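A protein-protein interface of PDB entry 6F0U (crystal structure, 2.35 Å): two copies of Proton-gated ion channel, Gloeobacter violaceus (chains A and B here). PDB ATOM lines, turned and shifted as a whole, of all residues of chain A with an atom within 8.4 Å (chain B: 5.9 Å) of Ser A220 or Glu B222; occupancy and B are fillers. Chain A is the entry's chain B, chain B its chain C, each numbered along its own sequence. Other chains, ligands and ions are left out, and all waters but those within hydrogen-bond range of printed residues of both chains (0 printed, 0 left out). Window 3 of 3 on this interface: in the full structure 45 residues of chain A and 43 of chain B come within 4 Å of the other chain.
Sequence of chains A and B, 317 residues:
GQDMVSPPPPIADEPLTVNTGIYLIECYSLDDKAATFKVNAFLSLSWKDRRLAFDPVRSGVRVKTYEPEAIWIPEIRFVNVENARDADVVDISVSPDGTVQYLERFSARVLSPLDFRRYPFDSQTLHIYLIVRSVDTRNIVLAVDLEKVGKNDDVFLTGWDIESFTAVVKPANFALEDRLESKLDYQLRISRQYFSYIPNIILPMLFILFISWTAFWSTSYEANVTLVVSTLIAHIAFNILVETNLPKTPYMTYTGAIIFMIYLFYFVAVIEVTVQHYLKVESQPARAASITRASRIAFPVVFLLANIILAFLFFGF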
ATOM      1  N   THR A 214     -15.926 -24.613  22.476  1.00  0.00           N
ATOM      2  CA  THR A 214     -15.236 -24.449  21.200  1.00  0.00           C
ATOM      3  C   THR A 214     -14.624 -25.795  20.783  1.00  0.00           C
ATOM      4  O   THR A 214     -14.357 -25.973  19.608  1.00  0.00           O
ATOM      5  CB  THR A 214     -14.195 -23.311  21.228  1.00  0.00           C
ATOM      6  OG1 THR A 214     -13.180 -23.620  22.180  1.00  0.00           O
ATOM      7  CG2 THR A 214     -14.804 -21.947  21.523  1.00  0.00           C
ATOM      8  N   ALA A 215     -14.460 -26.751  21.743  1.00  0.00           N
ATOM      9  CA  ALA A 215     -13.979 -28.119  21.517  1.00  0.00           C
ATOM     10  C   ALA A 215     -14.945 -28.896  20.585  1.00  0.00           C
ATOM     11  O   ALA A 215     -14.538 -29.892  19.981  1.00  0.00           O
ATOM     12  CB  ALA A 215     -13.820 -28.854  22.845  1.00  0.00           C
ATOM     13  N   TRP A 217     -16.030 -27.718  17.852  1.00  0.00           N
ATOM     14  CA  TRP A 217     -15.661 -27.258  16.519  1.00  0.00           C
ATOM     15  C   TRP A 217     -14.204 -27.627  16.210  1.00  0.00           C
ATOM     16  O   TRP A 217     -13.592 -27.038  15.313  1.00  0.00           O
ATOM     17  CB  TRP A 217     -15.921 -25.761  16.362  1.00  0.00           C
ATOM     18  CG  TRP A 217     -17.364 -25.444  16.135  1.00  0.00           C
ATOM     19  CD1 TRP A 217     -18.019 -25.361  14.933  1.00  0.00           C
ATOM     20  CD2 TRP A 217     -18.341 -25.186  17.149  1.00  0.00           C
ATOM     21  NE1 TRP A 217     -19.343 -25.042  15.141  1.00  0.00           N
ATOM     22  CE2 TRP A 217     -19.567 -24.924  16.494  1.00  0.00           C
ATOM     23  CE3 TRP A 217     -18.297 -25.142  18.554  1.00  0.00           C
ATOM     24  CZ2 TRP A 217     -20.739 -24.614  17.201  1.00  0.00           C
ATOM     25  CZ3 TRP A 217     -19.458 -24.858  19.255  1.00  0.00           C
ATOM     26  CH2 TRP A 217     -20.661 -24.587  18.583  1.00  0.00           C
ATOM     27  N   SER A 218     -13.668 -28.623  16.962  1.00  0.00           N
ATOM     28  CA  SER A 218     -12.315 -29.154  16.848  1.00  0.00           C
ATOM     29  C   SER A 218     -12.267 -30.679  16.938  1.00  0.00           C
ATOM     30  O   SER A 218     -12.946 -31.298  17.773  1.00  0.00           O
ATOM     31  CB  SER A 218     -11.416 -28.557  17.923  1.00  0.00           C
ATOM     32  OG  SER A 218     -10.194 -29.266  18.047  1.00  0.00           O
ATOM     33  N   THR A 219     -11.403 -31.268  16.083  1.00  0.00           N
ATOM     34  CA  THR A 219     -11.126 -32.704  15.991  1.00  0.00           C
ATOM     35  C   THR A 219      -9.815 -33.051  16.730  1.00  0.00           C
ATOM     36  O   THR A 219      -9.537 -34.237  16.974  1.00  0.00           O
ATOM     37  CB  THR A 219     -11.132 -33.171  14.518  1.00  0.00           C
ATOM     38  OG1 THR A 219     -10.370 -32.247  13.734  1.00  0.00           O
ATOM     39  CG2 THR A 219     -12.545 -33.273  13.941  1.00  0.00           C
ATOM     40  N   SER A 220      -9.030 -32.017  17.102  1.00  0.00           N
ATOM     41  CA  SER A 220      -7.773 -32.135  17.838  1.00  0.00           C
ATOM     42  C   SER A 220      -8.038 -32.488  19.310  1.00  0.00           C
ATOM     43  O   SER A 220      -8.352 -31.606  20.113  1.00  0.00           O
ATOM     44  CB  SER A 220      -6.977 -30.837  17.740  1.00  0.00           C
ATOM     45  OG  SER A 220      -5.786 -30.901  18.506  1.00  0.00           O
ATOM     46  N   TYR A 221      -7.896 -33.775  19.660  1.00  0.00           N
ATOM     47  CA  TYR A 221      -8.099 -34.286  21.011  1.00  0.00           C
ATOM     48  C   TYR A 221      -7.260 -33.554  22.060  1.00  0.00           C
ATOM     49  O   TYR A 221      -7.773 -33.213  23.123  1.00  0.00           O
ATOM     50  CB  TYR A 221      -7.810 -35.796  21.059  1.00  0.00           C
ATOM     51  CG  TYR A 221      -8.005 -36.441  22.419  1.00  0.00           C
ATOM     52  CD1 TYR A 221      -9.189 -36.267  23.134  1.00  0.00           C
ATOM     53  CD2 TYR A 221      -7.028 -37.263  22.970  1.00  0.00           C
ATOM     54  CE1 TYR A 221      -9.403 -36.917  24.351  1.00  0.00           C
ATOM     55  CE2 TYR A 221      -7.221 -37.896  24.199  1.00  0.00           C
ATOM     56  CZ  TYR A 221      -8.403 -37.707  24.894  1.00  0.00           C
ATOM     57  OH  TYR A 221      -8.583 -38.353  26.091  1.00  0.00           O
ATOM     58  N   GLU A 222      -5.981 -33.322  21.750  1.00  0.00           N
ATOM     59  CA  GLU A 222      -5.005 -32.679  22.629  1.00  0.00           C
ATOM     60  C   GLU A 222      -5.428 -31.235  22.967  1.00  0.00           C
ATOM     61  O   GLU A 222      -5.356 -30.826  24.130  1.00  0.00           O
ATOM     62  CB  GLU A 222      -3.590 -32.749  22.008  1.00  0.00           C
ATOM     63  CG  GLU A 222      -3.153 -34.138  21.491  1.00  0.00           C
ATOM     64  CD  GLU A 222      -3.751 -34.732  20.210  1.00  0.00           C
ATOM     65  OE1 GLU A 222      -4.016 -33.982  19.240  1.00  0.00           O
ATOM     66  OE2 GLU A 222      -3.920 -35.973  20.165  1.00  0.00           O
ATOM     67  N   ALA A 223      -5.919 -30.488  21.959  1.00  0.00           N
ATOM     68  CA  ALA A 223      -6.394 -29.118  22.117  1.00  0.00           C
ATOM     69  C   ALA A 223      -7.697 -29.095  22.915  1.00  0.00           C
ATOM     70  O   ALA A 223      -7.882 -28.224  23.767  1.00  0.00           O
ATOM     71  CB  ALA A 223      -6.602 -28.478  20.753  1.00  0.00           C
ATOM     72  N   ASN A 224      -8.590 -30.066  22.638  1.00  0.00           N
ATOM     73  CA  ASN A 224      -9.883 -30.251  23.300  1.00  0.00           C
ATOM     74  C   ASN A 224      -9.697 -30.501  24.776  1.00  0.00           C
ATOM     75  O   ASN A 224     -10.346 -29.840  25.588  1.00  0.00           O
ATOM     76  CB  ASN A 224     -10.649 -31.396  22.622  1.00  0.00           C
ATOM     77  CG  ASN A 224     -11.156 -31.003  21.278  1.00  0.00           C
ATOM     78  OD1 ASN A 224     -10.995 -29.855  20.855  1.00  0.00           O
ATOM     79  ND2 ASN A 224     -11.753 -31.943  20.564  1.00  0.00           N
ATOM     80  N   VAL A 225      -8.765 -31.414  25.122  1.00  0.00           N
ATOM     81  CA  VAL A 225      -8.393 -31.759  26.492  1.00  0.00           C
ATOM     82  C   VAL A 225      -7.876 -30.507  27.211  1.00  0.00           C
ATOM     83  O   VAL A 225      -8.332 -30.209  28.312  1.00  0.00           O
ATOM     84  CB  VAL A 225      -7.415 -32.965  26.506  1.00  0.00           C
ATOM     85  CG1 VAL A 225      -6.574 -33.006  27.775  1.00  0.00           C
ATOM     86  CG2 VAL A 225      -8.182 -34.259  26.340  1.00  0.00           C
ATOM     87  N   THR A 226      -7.009 -29.724  26.545  1.00  0.00           N
ATOM     88  CA  THR A 226      -6.471 -28.470  27.083  1.00  0.00           C
ATOM     89  C   THR A 226      -7.611 -27.455  27.309  1.00  0.00           C
ATOM     90  O   THR A 226      -7.654 -26.824  28.349  1.00  0.00           O
ATOM     91  CB  THR A 226      -5.344 -27.940  26.167  1.00  0.00           C
ATOM     92  OG1 THR A 226      -4.288 -28.895  26.150  1.00  0.00           O
ATOM     93  CG2 THR A 226      -4.791 -26.598  26.622  1.00  0.00           C
ATOM     94  N   LEU A 227      -8.540 -27.334  26.350  1.00  0.00           N
ATOM     95  CA  LEU A 227      -9.671 -26.423  26.453  1.00  0.00           C
ATOM     96  C   LEU A 227     -10.595 -26.735  27.634  1.00  0.00           C
ATOM     97  O   LEU A 227     -10.892 -25.842  28.411  1.00  0.00           O
ATOM     98  CB  LEU A 227     -10.492 -26.424  25.151  1.00  0.00           C
ATOM     99  CG  LEU A 227     -10.029 -25.491  24.052  1.00  0.00           C
ATOM    100  CD1 LEU A 227     -10.441 -26.020  22.672  1.00  0.00           C
ATOM    101  CD2 LEU A 227     -10.526 -24.076  24.282  1.00  0.00           C
ATOM    102  N   VAL A 273     -15.581 -35.325  24.238  1.00  0.00           N
ATOM    103  CA  VAL A 273     -14.216 -35.186  23.720  1.00  0.00           C
ATOM    104  C   VAL A 273     -13.509 -36.557  23.687  1.00  0.00           C
ATOM    105  O   VAL A 273     -12.806 -36.844  22.720  1.00  0.00           O
ATOM    106  CB  VAL A 273     -13.465 -34.093  24.545  1.00  0.00           C
ATOM    107  CG1 VAL A 273     -11.948 -34.251  24.499  1.00  0.00           C
ATOM    108  CG2 VAL A 273     -13.881 -32.698  24.098  1.00  0.00           C
ATOM    109  N   GLN A 276     -15.488 -38.897  21.051  1.00  0.00           N
ATOM    110  CA  GLN A 276     -15.082 -38.373  19.745  1.00  0.00           C
ATOM    111  C   GLN A 276     -13.716 -38.918  19.339  1.00  0.00           C
ATOM    112  O   GLN A 276     -13.580 -39.439  18.234  1.00  0.00           O
ATOM    113  CB  GLN A 276     -15.067 -36.838  19.755  1.00  0.00           C
ATOM    114  CG  GLN A 276     -14.652 -36.194  18.420  1.00  0.00           C
ATOM    115  CD  GLN A 276     -14.163 -34.762  18.574  1.00  0.00           C
ATOM    116  OE1 GLN A 276     -13.531 -34.372  19.585  1.00  0.00           O
ATOM    117  NE2 GLN A 276     -14.424 -33.956  17.552  1.00  0.00           N
ATOM    118  N   HIS A 277     -12.721 -38.816  20.234  1.00  0.00           N
ATOM    119  CA  HIS A 277     -11.365 -39.297  19.984  1.00  0.00           C
ATOM    120  C   HIS A 277     -11.313 -40.821  19.793  1.00  0.00           C
ATOM    121  O   HIS A 277     -10.661 -41.289  18.858  1.00  0.00           O
ATOM    122  CB  HIS A 277     -10.447 -38.854  21.122  1.00  0.00           C
ATOM    123  CG  HIS A 277      -9.053 -39.381  21.021  1.00  0.00           C
ATOM    124  ND1 HIS A 277      -8.201 -38.973  20.013  1.00  0.00           N
ATOM    125  CD2 HIS A 277      -8.406 -40.264  21.812  1.00  0.00           C
ATOM    126  CE1 HIS A 277      -7.064 -39.609  20.229  1.00  0.00           C
ATOM    127  NE2 HIS A 277      -7.142 -40.400  21.297  1.00  0.00           N
ATOM    128  N   LYS A 280     -12.688 -41.750  16.390  1.00  0.00           N
ATOM    129  CA  LYS A 280     -11.738 -41.359  15.341  1.00  0.00           C
ATOM    130  C   LYS A 280     -10.628 -42.401  15.213  1.00  0.00           C
ATOM    131  O   LYS A 280     -10.302 -42.817  14.100  1.00  0.00           O
ATOM    132  CB  LYS A 280     -11.141 -39.962  15.617  1.00  0.00           C
ATOM    133  CG  LYS A 280     -12.131 -38.801  15.463  1.00  0.00           C
ATOM    134  CD  LYS A 280     -12.040 -38.111  14.110  1.00  0.00           C
ATOM    135  CE  LYS A 280     -12.927 -36.900  14.009  1.00  0.00           C
ATOM    136  NZ  LYS A 280     -14.367 -37.239  13.980  1.00  0.00           N
ATOM    137  N   SER B 220      -0.332 -23.054  14.446  1.00  0.00           N
ATOM    138  CA  SER B 220      -0.401 -24.166  15.393  1.00  0.00           C
ATOM    139  C   SER B 220      -1.554 -23.970  16.368  1.00  0.00           C
ATOM    140  O   SER B 220      -1.419 -23.229  17.342  1.00  0.00           O
ATOM    141  CB  SER B 220       0.921 -24.310  16.145  1.00  0.00           C
ATOM    142  OG  SER B 220       0.862 -25.329  17.131  1.00  0.00           O
ATOM    143  N   TYR B 221      -2.681 -24.653  16.116  1.00  0.00           N
ATOM    144  CA  TYR B 221      -3.881 -24.593  16.943  1.00  0.00           C
ATOM    145  C   TYR B 221      -3.612 -24.914  18.419  1.00  0.00           C
ATOM    146  O   TYR B 221      -4.105 -24.213  19.302  1.00  0.00           O
ATOM    147  CB  TYR B 221      -4.960 -25.534  16.379  1.00  0.00           C
ATOM    148  CG  TYR B 221      -6.260 -25.546  17.159  1.00  0.00           C
ATOM    149  CD1 TYR B 221      -6.922 -24.360  17.469  1.00  0.00           C
ATOM    150  CD2 TYR B 221      -6.854 -26.745  17.545  1.00  0.00           C
ATOM    151  CE1 TYR B 221      -8.152 -24.368  18.116  1.00  0.00           C
ATOM    152  CE2 TYR B 221      -8.073 -26.761  18.219  1.00  0.00           C
ATOM    153  CZ  TYR B 221      -8.705 -25.568  18.520  1.00  0.00           C
ATOM    154  OH  TYR B 221      -9.891 -25.572  19.190  1.00  0.00           O
ATOM    155  N   GLU B 222      -2.836 -25.978  18.667  1.00  0.00           N
ATOM    156  CA  GLU B 222      -2.486 -26.468  19.994  1.00  0.00           C
ATOM    157  C   GLU B 222      -1.715 -25.405  20.789  1.00  0.00           C
ATOM    158  O   GLU B 222      -2.010 -25.190  21.966  1.00  0.00           O
ATOM    159  CB  GLU B 222      -1.710 -27.804  19.908  1.00  0.00           C
ATOM    160  CG  GLU B 222      -2.318 -28.882  18.991  1.00  0.00           C
ATOM    161  CD  GLU B 222      -2.288 -28.722  17.467  1.00  0.00           C
ATOM    162  OE1 GLU B 222      -1.279 -28.222  16.920  1.00  0.00           O
ATOM    163  OE2 GLU B 222      -3.276 -29.136  16.814  1.00  0.00           O
ATOM    164  N   ALA B 223      -0.759 -24.721  20.137  1.00  0.00           N
ATOM    165  CA  ALA B 223       0.046 -23.663  20.752  1.00  0.00           C
ATOM    166  C   ALA B 223      -0.815 -22.428  21.034  1.00  0.00           C
ATOM    167  O   ALA B 223      -0.673 -21.799  22.080  1.00  0.00           O
ATOM    168  CB  ALA B 223       1.211 -23.300  19.849  1.00  0.00           C
ATOM    169  N   ASN B 224      -1.711 -22.098  20.083  1.00  0.00           N
ATOM    170  CA  ASN B 224      -2.653 -20.982  20.152  1.00  0.00           C
ATOM    171  C   ASN B 224      -3.589 -21.144  21.325  1.00  0.00           C
ATOM    172  O   ASN B 224      -3.742 -20.207  22.107  1.00  0.00           O
ATOM    173  CB  ASN B 224      -3.424 -20.868  18.829  1.00  0.00           C
ATOM    174  CG  ASN B 224      -2.561 -20.366  17.727  1.00  0.00           C
ATOM    175  OD1 ASN B 224      -1.401 -20.025  17.949  1.00  0.00           O
ATOM    176  ND2 ASN B 224      -3.091 -20.335  16.509  1.00  0.00           N
ATOM    177  N   VAL B 225      -4.162 -22.355  21.483  1.00  0.00           N
ATOM    178  CA  VAL B 225      -5.050 -22.733  22.578  1.00  0.00           C
ATOM    179  C   VAL B 225      -4.308 -22.571  23.904  1.00  0.00           C
ATOM    180  O   VAL B 225      -4.846 -21.947  24.815  1.00  0.00           O
ATOM    181  CB  VAL B 225      -5.642 -24.140  22.340  1.00  0.00           C
ATOM    182  CG1 VAL B 225      -6.070 -24.811  23.640  1.00  0.00           C
ATOM    183  CG2 VAL B 225      -6.806 -24.058  21.370  1.00  0.00           C
ATOM    184  N   THR B 226      -3.049 -23.040  23.977  1.00  0.00           N
ATOM    185  CA  THR B 226      -2.191 -22.911  25.162  1.00  0.00           C
ATOM    186  C   THR B 226      -1.931 -21.433  25.463  1.00  0.00           C
ATOM    187  O   THR B 226      -2.055 -21.030  26.612  1.00  0.00           O
ATOM    188  CB  THR B 226      -0.905 -23.740  24.997  1.00  0.00           C
ATOM    189  OG1 THR B 226      -1.257 -25.112  24.843  1.00  0.00           O
ATOM    190  CG2 THR B 226       0.055 -23.594  26.165  1.00  0.00           C
ATOM    191  N   LEU B 227      -1.621 -20.627  24.435  1.00  0.00           N
ATOM    192  CA  LEU B 227      -1.365 -19.196  24.592  1.00  0.00           C
ATOM    193  C   LEU B 227      -2.565 -18.426  25.149  1.00  0.00           C
ATOM    194  O   LEU B 227      -2.401 -17.699  26.116  1.00  0.00           O
ATOM    195  CB  LEU B 227      -0.940 -18.572  23.249  1.00  0.00           C
ATOM    196  CG  LEU B 227       0.532 -18.640  22.904  1.00  0.00           C
ATOM    197  CD1 LEU B 227       0.741 -18.601  21.399  1.00  0.00           C
ATOM    198  CD2 LEU B 227       1.311 -17.536  23.587  1.00  0.00           C
ATOM    199  N   HIS B 277      -8.468 -22.643  12.784  1.00  0.00           N
ATOM    200  CA  HIS B 277      -8.246 -24.084  12.790  1.00  0.00           C
ATOM    201  C   HIS B 277      -9.286 -24.836  11.949  1.00  0.00           C
ATOM    202  O   HIS B 277      -8.911 -25.695  11.154  1.00  0.00           O
ATOM    203  CB  HIS B 277      -8.236 -24.603  14.228  1.00  0.00           C
ATOM    204  CG  HIS B 277      -8.103 -26.091  14.336  1.00  0.00           C
ATOM    205  ND1 HIS B 277      -6.943 -26.748  13.940  1.00  0.00           N
ATOM    206  CD2 HIS B 277      -8.987 -27.004  14.791  1.00  0.00           C
ATOM    207  CE1 HIS B 277      -7.161 -28.030  14.177  1.00  0.00           C
ATOM    208  NE2 HIS B 277      -8.379 -28.235  14.677  1.00  0.00           N
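The backbone NH (N) of Ser A220 lies within hydrogen-bond range of the side-chain hydroxyl (OG) of Ser A218, 3.1 Å away.
The backbone NH (N) of Ala A223 sits close to the side-chain hydroxyl (OG) of Ser A220.
OG1 of Thr A226 sits at hydrogen-bond distance from O of Glu A222, at 3.0 Å.
The side-chain hydroxyl (OG) of Ser A218 is in hydrogen-bond range of the side-chain amide oxygen (OD1) of Asn A224 (3.0 Å).
The backbone carbonyl oxygen (O) of Glu B222 is in hydrogen-bond range of the side-chain hydroxyl (OG1) of Thr B226 (3.0 Å).
O of Ser A220 lies close to OD1 of Asn A224 (3.3 Å).
Among the printed residues, merely in contact across the chains: Ser A218 with Tyr B221 (3.3 Å), Ala A223 with Tyr B221 (3.4 Å), Ser A220 with Glu B222 (3.5 Å), Leu A227 with Tyr B221 (3.6 Å), Thr A226 with Val B225 (3.7 Å), Ala A223 with Val B225 (3.9 Å) and Ser A218 with His B277 (3.96 Å).
Of the printed residues of chain B, Ser A218 touches Tyr B221 and His B277.
Ser A220 touches just one residue of chain B: Glu B222 (3.5 Å).
Of the printed residues of chain B, Thr A226 touches Val B225 (3.7 Å).
Of the printed residues of chain A, Tyr B221 touches Ser A218, Ala A223 and Leu A227.
Glu B222 touches one residue of chain A.
Ala B223 touches none of the printed residues of chain A.
Printed residues of chain A within 4 Å of Val B225: Ala A223 (3.9 Å) and Thr A226 (3.7 Å).
The nearest printed residue of chain A that does not touch Val B225 is Leu A227 (4.04 Å).
Hydrophobic or aromatic side chains of chain A within 4 Å of the printed part of chain B: Ala A223 and Leu A227.
Among the printed residues, 7 pairs touch across the chains.
Among the printed residues, no Asp or Glu carboxylate lies within 4 Å of a Lys or Arg side-chain nitrogen of the other chain.
Ala A223 touches Tyr B221, but with the chains exchanged Tyr A221 does not touch Ala B223 (11.1 Å).
Ala A223 touches Val B225, but with the chains exchanged Val A225 does not touch Ala B223 (11.6 Å).
Thr A226 touches Val B225, but with the chains exchanged Val A225 does not touch Thr B226 (8.9 Å).
Leu A227 touches Tyr B221, but with the chains exchanged Tyr A221 does not touch Leu B227 (14.1 Å).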
